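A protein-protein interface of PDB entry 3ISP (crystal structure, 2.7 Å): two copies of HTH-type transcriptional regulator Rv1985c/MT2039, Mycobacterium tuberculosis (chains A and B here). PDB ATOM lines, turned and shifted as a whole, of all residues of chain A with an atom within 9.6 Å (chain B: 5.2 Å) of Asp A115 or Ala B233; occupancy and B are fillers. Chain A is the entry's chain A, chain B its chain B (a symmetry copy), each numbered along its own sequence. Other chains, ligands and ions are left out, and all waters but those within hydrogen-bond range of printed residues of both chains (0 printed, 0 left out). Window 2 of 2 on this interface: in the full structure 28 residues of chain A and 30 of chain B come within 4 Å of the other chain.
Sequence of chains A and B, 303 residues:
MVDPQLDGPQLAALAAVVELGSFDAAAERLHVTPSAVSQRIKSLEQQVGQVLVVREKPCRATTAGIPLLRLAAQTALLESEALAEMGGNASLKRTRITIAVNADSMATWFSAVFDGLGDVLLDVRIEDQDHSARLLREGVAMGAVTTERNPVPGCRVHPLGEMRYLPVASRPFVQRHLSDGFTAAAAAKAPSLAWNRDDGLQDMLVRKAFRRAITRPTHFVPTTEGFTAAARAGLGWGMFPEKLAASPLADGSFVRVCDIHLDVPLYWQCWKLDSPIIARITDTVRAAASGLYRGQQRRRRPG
The backbone NH (N) of Leu B235 sits close to the backbone carbonyl oxygen (O) of Ala B230.
Among the printed residues, merely in contact across the chains: Ser A111 with Ala B229 (3.3 Å), Phe A114 with Ala B229 (3.8 Å), Phe A114 with Ala B230 (3.6 Å), Phe A114 with Ala B233 (3.9 Å), Phe A114 with Leu B235 (3.3 Å) and Asp A115 with Ala B233 (3.1 Å).
Of chain B, only Ala B233 (3.1 Å) comes within 4 Å of Asp A115.
Printed residues of chain B within 4 Å of Ser A111: Ala B229 (3.3 Å).
Printed residues of chain A within 4 Å of Leu B235: Phe A114 (3.3 Å).
Printed residues of chain A within 4 Å of Ala B229: Ser A111 (3.3 Å) and Phe A114 (3.8 Å).
The nearest residue of chain A that does not touch Ala B233 is Ser A111 (5.9 Å).
Printed residues of chain A that touch a printed residue of chain B: Ser A111, Phe A114 and Asp A115.
Hydrophobic or aromatic side chains of chain A within 4 Å of the printed part of chain B: Phe A114.
Along chain A the printed residues that touch a printed residue of chain B span positions 111 to 115.
Of the 9 printed residues of chain B, 4 touch a printed residue of chain A.
Hydrophobic or aromatic side chains of chain B that line the printed part of chain A: Ala B229, Ala B233 and Leu B235.
Along chain B the printed residues that touch a printed residue of chain A span positions 229 to 235.
Among the printed residues, no Asp or Glu carboxylate lies within 4 Å of a Lys or Arg side-chain nitrogen of the other chain.
No position is printed for both chains.
Of the 6 pairs that touch across the chains among the printed residues, none has its exchanged pair printed and touching as well.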
ATOM      1  N   ARG A  94      -8.468 -20.675  -4.844  1.00  0.00           N
ATOM      2  CA  ARG A  94      -7.566 -21.428  -3.982  1.00  0.00           C
ATOM      3  C   ARG A  94      -6.180 -20.797  -3.963  1.00  0.00           C
ATOM      4  O   ARG A  94      -5.350 -21.064  -4.834  1.00  0.00           O
ATOM      5  CB  ARG A  94      -7.512 -22.904  -4.386  1.00  0.00           C
ATOM      6  CG  ARG A  94      -8.383 -23.767  -3.495  1.00  0.00           C
ATOM      7  CD  ARG A  94      -8.417 -23.138  -2.102  1.00  0.00           C
ATOM      8  NE  ARG A  94      -8.759 -24.041  -1.001  1.00  0.00           N
ATOM      9  CZ  ARG A  94      -8.486 -25.344  -0.949  1.00  0.00           C
ATOM     10  NH1 ARG A  94      -7.849 -25.949  -1.943  1.00  0.00           N
ATOM     11  NH2 ARG A  94      -8.851 -26.049   0.115  1.00  0.00           N
ATOM     12  N   THR A 108       3.820 -29.783  18.096  1.00  0.00           N
ATOM     13  CA  THR A 108       2.951 -29.572  19.235  1.00  0.00           C
ATOM     14  C   THR A 108       1.705 -28.791  18.842  1.00  0.00           C
ATOM     15  O   THR A 108       0.768 -29.345  18.270  1.00  0.00           O
ATOM     16  CB  THR A 108       3.690 -28.895  20.388  1.00  0.00           C
ATOM     17  OG1 THR A 108       4.222 -27.643  19.946  1.00  0.00           O
ATOM     18  CG2 THR A 108       4.836 -29.768  20.854  1.00  0.00           C
ATOM     19  N   TRP A 109       1.706 -27.495  19.107  1.00  0.00           N
ATOM     20  CA  TRP A 109       0.489 -26.715  18.960  1.00  0.00           C
ATOM     21  C   TRP A 109       0.070 -26.390  17.532  1.00  0.00           C
ATOM     22  O   TRP A 109      -1.128 -26.395  17.243  1.00  0.00           O
ATOM     23  CB  TRP A 109       0.587 -25.449  19.788  1.00  0.00           C
ATOM     24  CG  TRP A 109       1.665 -24.532  19.361  1.00  0.00           C
ATOM     25  CD1 TRP A 109       2.961 -24.514  19.794  1.00  0.00           C
ATOM     26  CD2 TRP A 109       1.538 -23.461  18.423  1.00  0.00           C
ATOM     27  NE1 TRP A 109       3.655 -23.500  19.166  1.00  0.00           N
ATOM     28  CE2 TRP A 109       2.802 -22.838  18.324  1.00  0.00           C
ATOM     29  CE3 TRP A 109       0.478 -22.969  17.657  1.00  0.00           C
ATOM     30  CZ2 TRP A 109       3.029 -21.755  17.495  1.00  0.00           C
ATOM     31  CZ3 TRP A 109       0.706 -21.898  16.839  1.00  0.00           C
ATOM     32  CH2 TRP A 109       1.973 -21.298  16.760  1.00  0.00           C
ATOM     33  N   PHE A 110       1.026 -26.127  16.637  1.00  0.00           N
ATOM     34  CA  PHE A 110       0.687 -25.581  15.314  1.00  0.00           C
ATOM     35  C   PHE A 110      -0.277 -26.448  14.509  1.00  0.00           C
ATOM     36  O   PHE A 110      -1.069 -25.949  13.719  1.00  0.00           O
ATOM     37  CB  PHE A 110       1.940 -25.302  14.489  1.00  0.00           C
ATOM     38  CG  PHE A 110       1.698 -24.419  13.288  1.00  0.00           C
ATOM     39  CD1 PHE A 110       1.911 -23.060  13.358  1.00  0.00           C
ATOM     40  CD2 PHE A 110       1.270 -24.955  12.086  1.00  0.00           C
ATOM     41  CE1 PHE A 110       1.690 -22.258  12.254  1.00  0.00           C
ATOM     42  CE2 PHE A 110       1.057 -24.153  10.985  1.00  0.00           C
ATOM     43  CZ  PHE A 110       1.261 -22.810  11.069  1.00  0.00           C
ATOM     44  N   SER A 111      -0.186 -27.753  14.701  1.00  0.00           N
ATOM     45  CA  SER A 111      -1.072 -28.694  14.042  1.00  0.00           C
ATOM     46  C   SER A 111      -2.507 -28.184  13.915  1.00  0.00           C
ATOM     47  O   SER A 111      -3.171 -28.430  12.918  1.00  0.00           O
ATOM     48  CB  SER A 111      -1.074 -29.998  14.826  1.00  0.00           C
ATOM     49  OG  SER A 111      -2.140 -30.814  14.398  1.00  0.00           O
ATOM     50  N   ALA A 112      -2.984 -27.474  14.931  1.00  0.00           N
ATOM     51  CA  ALA A 112      -4.388 -27.076  15.006  1.00  0.00           C
ATOM     52  C   ALA A 112      -4.796 -26.185  13.855  1.00  0.00           C
ATOM     53  O   ALA A 112      -5.981 -26.082  13.540  1.00  0.00           O
ATOM     54  CB  ALA A 112      -4.674 -26.377  16.338  1.00  0.00           C
ATOM     55  N   VAL A 113      -3.813 -25.544  13.228  1.00  0.00           N
ATOM     56  CA  VAL A 113      -4.070 -24.495  12.239  1.00  0.00           C
ATOM     57  C   VAL A 113      -4.753 -25.026  10.987  1.00  0.00           C
ATOM     58  O   VAL A 113      -5.436 -24.278  10.283  1.00  0.00           O
ATOM     59  CB  VAL A 113      -2.766 -23.768  11.835  1.00  0.00           C
ATOM     60  CG1 VAL A 113      -3.024 -22.761  10.724  1.00  0.00           C
ATOM     61  CG2 VAL A 113      -2.138 -23.086  13.041  1.00  0.00           C
ATOM     62  N   PHE A 114      -4.563 -26.317  10.709  1.00  0.00           N
ATOM     63  CA  PHE A 114      -5.143 -26.927   9.514  1.00  0.00           C
ATOM     64  C   PHE A 114      -6.644 -27.071   9.680  1.00  0.00           C
ATOM     65  O   PHE A 114      -7.403 -26.882   8.734  1.00  0.00           O
ATOM     66  CB  PHE A 114      -4.537 -28.307   9.240  1.00  0.00           C
ATOM     67  CG  PHE A 114      -3.050 -28.302   9.053  1.00  0.00           C
ATOM     68  CD1 PHE A 114      -2.428 -27.300   8.347  1.00  0.00           C
ATOM     69  CD2 PHE A 114      -2.277 -29.318   9.569  1.00  0.00           C
ATOM     70  CE1 PHE A 114      -1.062 -27.306   8.179  1.00  0.00           C
ATOM     71  CE2 PHE A 114      -0.909 -29.329   9.396  1.00  0.00           C
ATOM     72  CZ  PHE A 114      -0.303 -28.330   8.699  1.00  0.00           C
ATOM     73  N   ASP A 115      -7.063 -27.413  10.891  1.00  0.00           N
ATOM     74  CA  ASP A 115      -8.467 -27.679  11.164  1.00  0.00           C
ATOM     75  C   ASP A 115      -9.310 -26.454  10.893  1.00  0.00           C
ATOM     76  O   ASP A 115     -10.390 -26.548  10.313  1.00  0.00           O
ATOM     77  CB  ASP A 115      -8.646 -28.136  12.610  1.00  0.00           C
ATOM     78  CG  ASP A 115      -7.935 -29.448  12.891  1.00  0.00           C
ATOM     79  OD1 ASP A 115      -7.130 -29.500  13.854  1.00  0.00           O
ATOM     80  OD2 ASP A 115      -8.170 -30.420  12.133  1.00  0.00           O
ATOM     81  N   GLY A 116      -8.801 -25.300  11.307  1.00  0.00           N
ATOM     82  CA  GLY A 116      -9.494 -24.046  11.108  1.00  0.00           C
ATOM     83  C   GLY A 116      -8.949 -23.323   9.905  1.00  0.00           C
ATOM     84  O   GLY A 116      -8.689 -22.125   9.951  1.00  0.00           O
ATOM     85  N   LEU A 117      -8.788 -24.041   8.807  1.00  0.00           N
ATOM     86  CA  LEU A 117      -8.193 -23.428   7.626  1.00  0.00           C
ATOM     87  C   LEU A 117      -9.034 -23.549   6.355  1.00  0.00           C
ATOM     88  O   LEU A 117      -9.665 -24.582   6.092  1.00  0.00           O
ATOM     89  CB  LEU A 117      -6.801 -24.007   7.372  1.00  0.00           C
ATOM     90  CG  LEU A 117      -5.834 -23.090   6.628  1.00  0.00           C
ATOM     91  CD1 LEU A 117      -4.787 -22.552   7.596  1.00  0.00           C
ATOM     92  CD2 LEU A 117      -5.177 -23.858   5.502  1.00  0.00           C
ATOM     93  N   GLY A 118      -9.014 -22.480   5.567  1.00  0.00           N
ATOM     94  CA  GLY A 118      -9.691 -22.448   4.286  1.00  0.00           C
ATOM     95  C   GLY A 118      -9.987 -21.020   3.877  1.00  0.00           C
ATOM     96  O   GLY A 118      -9.956 -20.107   4.709  1.00  0.00           O
ATOM     97  N   LEU A 122      -1.950 -24.703   1.196  1.00  0.00           N
ATOM     98  CA  LEU A 122      -0.896 -24.528   2.189  1.00  0.00           C
ATOM     99  C   LEU A 122       0.475 -25.045   1.725  1.00  0.00           C
ATOM    100  O   LEU A 122       0.595 -26.153   1.200  1.00  0.00           O
ATOM    101  CB  LEU A 122      -1.312 -25.241   3.470  1.00  0.00           C
ATOM    102  CG  LEU A 122      -0.999 -24.560   4.796  1.00  0.00           C
ATOM    103  CD1 LEU A 122      -1.093 -23.051   4.675  1.00  0.00           C
ATOM    104  CD2 LEU A 122      -1.966 -25.051   5.840  1.00  0.00           C
ATOM    105  N   THR A 284      -5.900 -17.528  13.133  1.00  0.00           N
ATOM    106  CA  THR A 284      -5.801 -18.956  13.328  1.00  0.00           C
ATOM    107  C   THR A 284      -4.502 -19.336  14.045  1.00  0.00           C
ATOM    108  O   THR A 284      -4.525 -20.043  15.045  1.00  0.00           O
ATOM    109  CB  THR A 284      -5.929 -19.663  12.000  1.00  0.00           C
ATOM    110  OG1 THR A 284      -7.245 -19.421  11.497  1.00  0.00           O
ATOM    111  CG2 THR A 284      -5.707 -21.155  12.165  1.00  0.00           C
ATOM    112  N   ALA A 288      -4.290 -21.022  17.719  1.00  0.00           N
ATOM    113  CA  ALA A 288      -3.698 -22.337  17.856  1.00  0.00           C
ATOM    114  C   ALA A 288      -2.673 -22.310  18.991  1.00  0.00           C
ATOM    115  O   ALA A 288      -2.332 -23.348  19.586  1.00  0.00           O
ATOM    116  CB  ALA A 288      -3.053 -22.760  16.554  1.00  0.00           C
ATOM    117  N   SER B 170      -9.020 -38.876   5.221  1.00  0.00           N
ATOM    118  CA  SER B 170      -9.855 -39.089   6.398  1.00  0.00           C
ATOM    119  C   SER B 170     -11.221 -39.563   5.938  1.00  0.00           C
ATOM    120  O   SER B 170     -11.551 -39.448   4.756  1.00  0.00           O
ATOM    121  CB  SER B 170     -10.016 -37.787   7.168  1.00  0.00           C
ATOM    122  OG  SER B 170     -10.586 -36.796   6.326  1.00  0.00           O
ATOM    123  N   THR B 228       0.944 -35.719   8.686  1.00  0.00           N
ATOM    124  CA  THR B 228      -0.091 -36.594   9.217  1.00  0.00           C
ATOM    125  C   THR B 228      -1.275 -35.752   9.696  1.00  0.00           C
ATOM    126  O   THR B 228      -2.426 -36.102   9.465  1.00  0.00           O
ATOM    127  CB  THR B 228       0.452 -37.503  10.366  1.00  0.00           C
ATOM    128  OG1 THR B 228      -0.413 -38.628  10.560  1.00  0.00           O
ATOM    129  CG2 THR B 228       0.550 -36.749  11.674  1.00  0.00           C
ATOM    130  N   ALA B 229      -0.980 -34.627  10.342  1.00  0.00           N
ATOM    131  CA  ALA B 229      -2.014 -33.750  10.893  1.00  0.00           C
ATOM    132  C   ALA B 229      -2.855 -33.100   9.794  1.00  0.00           C
ATOM    133  O   ALA B 229      -4.058 -32.870   9.964  1.00  0.00           O
ATOM    134  CB  ALA B 229      -1.384 -32.687  11.780  1.00  0.00           C
ATOM    135  N   ALA B 230      -2.207 -32.799   8.676  1.00  0.00           N
ATOM    136  CA  ALA B 230      -2.885 -32.265   7.515  1.00  0.00           C
ATOM    137  C   ALA B 230      -3.972 -33.237   7.040  1.00  0.00           C
ATOM    138  O   ALA B 230      -5.157 -32.896   7.022  1.00  0.00           O
ATOM    139  CB  ALA B 230      -1.887 -31.985   6.420  1.00  0.00           C
ATOM    140  N   ALA B 231      -3.567 -34.456   6.683  1.00  0.00           N
ATOM    141  CA  ALA B 231      -4.506 -35.483   6.223  1.00  0.00           C
ATOM    142  C   ALA B 231      -5.604 -35.786   7.235  1.00  0.00           C
ATOM    143  O   ALA B 231      -6.766 -35.960   6.875  1.00  0.00           O
ATOM    144  CB  ALA B 231      -3.766 -36.750   5.880  1.00  0.00           C
ATOM    145  N   ARG B 232      -5.229 -35.868   8.503  1.00  0.00           N
ATOM    146  CA  ARG B 232      -6.206 -36.131   9.545  1.00  0.00           C
ATOM    147  C   ARG B 232      -7.259 -35.026   9.530  1.00  0.00           C
ATOM    148  O   ARG B 232      -8.433 -35.268   9.809  1.00  0.00           O
ATOM    149  CB  ARG B 232      -5.522 -36.239  10.913  1.00  0.00           C
ATOM    150  CG  ARG B 232      -6.306 -37.053  11.938  1.00  0.00           C
ATOM    151  CD  ARG B 232      -7.483 -36.259  12.502  1.00  0.00           C
ATOM    152  NE  ARG B 232      -8.473 -37.117  13.151  1.00  0.00           N
ATOM    153  CZ  ARG B 232      -8.434 -37.476  14.431  1.00  0.00           C
ATOM    154  NH1 ARG B 232      -7.447 -37.052  15.214  1.00  0.00           N
ATOM    155  NH2 ARG B 232      -9.383 -38.263  14.930  1.00  0.00           N
ATOM    156  N   ALA B 233      -6.829 -33.818   9.175  1.00  0.00           N
ATOM    157  CA  ALA B 233      -7.717 -32.663   9.143  1.00  0.00           C
ATOM    158  C   ALA B 233      -8.468 -32.553   7.819  1.00  0.00           C
ATOM    159  O   ALA B 233      -8.755 -31.453   7.349  1.00  0.00           O
ATOM    160  CB  ALA B 233      -6.931 -31.394   9.408  1.00  0.00           C
ATOM    161  N   GLY B 234      -8.785 -33.697   7.221  1.00  0.00           N
ATOM    162  CA  GLY B 234      -9.479 -33.730   5.942  1.00  0.00           C
ATOM    163  C   GLY B 234      -8.939 -32.739   4.922  1.00  0.00           C
ATOM    164  O   GLY B 234      -9.678 -32.257   4.066  1.00  0.00           O
ATOM    165  N   LEU B 235      -7.646 -32.455   5.003  1.00  0.00           N
ATOM    166  CA  LEU B 235      -7.032 -31.402   4.206  1.00  0.00           C
ATOM    167  C   LEU B 235      -6.525 -31.908   2.856  1.00  0.00           C
ATOM    168  O   LEU B 235      -6.147 -31.124   1.991  1.00  0.00           O
ATOM    169  CB  LEU B 235      -5.883 -30.773   5.002  1.00  0.00           C
ATOM    170  CG  LEU B 235      -5.580 -29.275   4.902  1.00  0.00           C
ATOM    171  CD1 LEU B 235      -4.588 -28.874   5.988  1.00  0.00           C
ATOM    172  CD2 LEU B 235      -5.034 -28.937   3.544  1.00  0.00           C
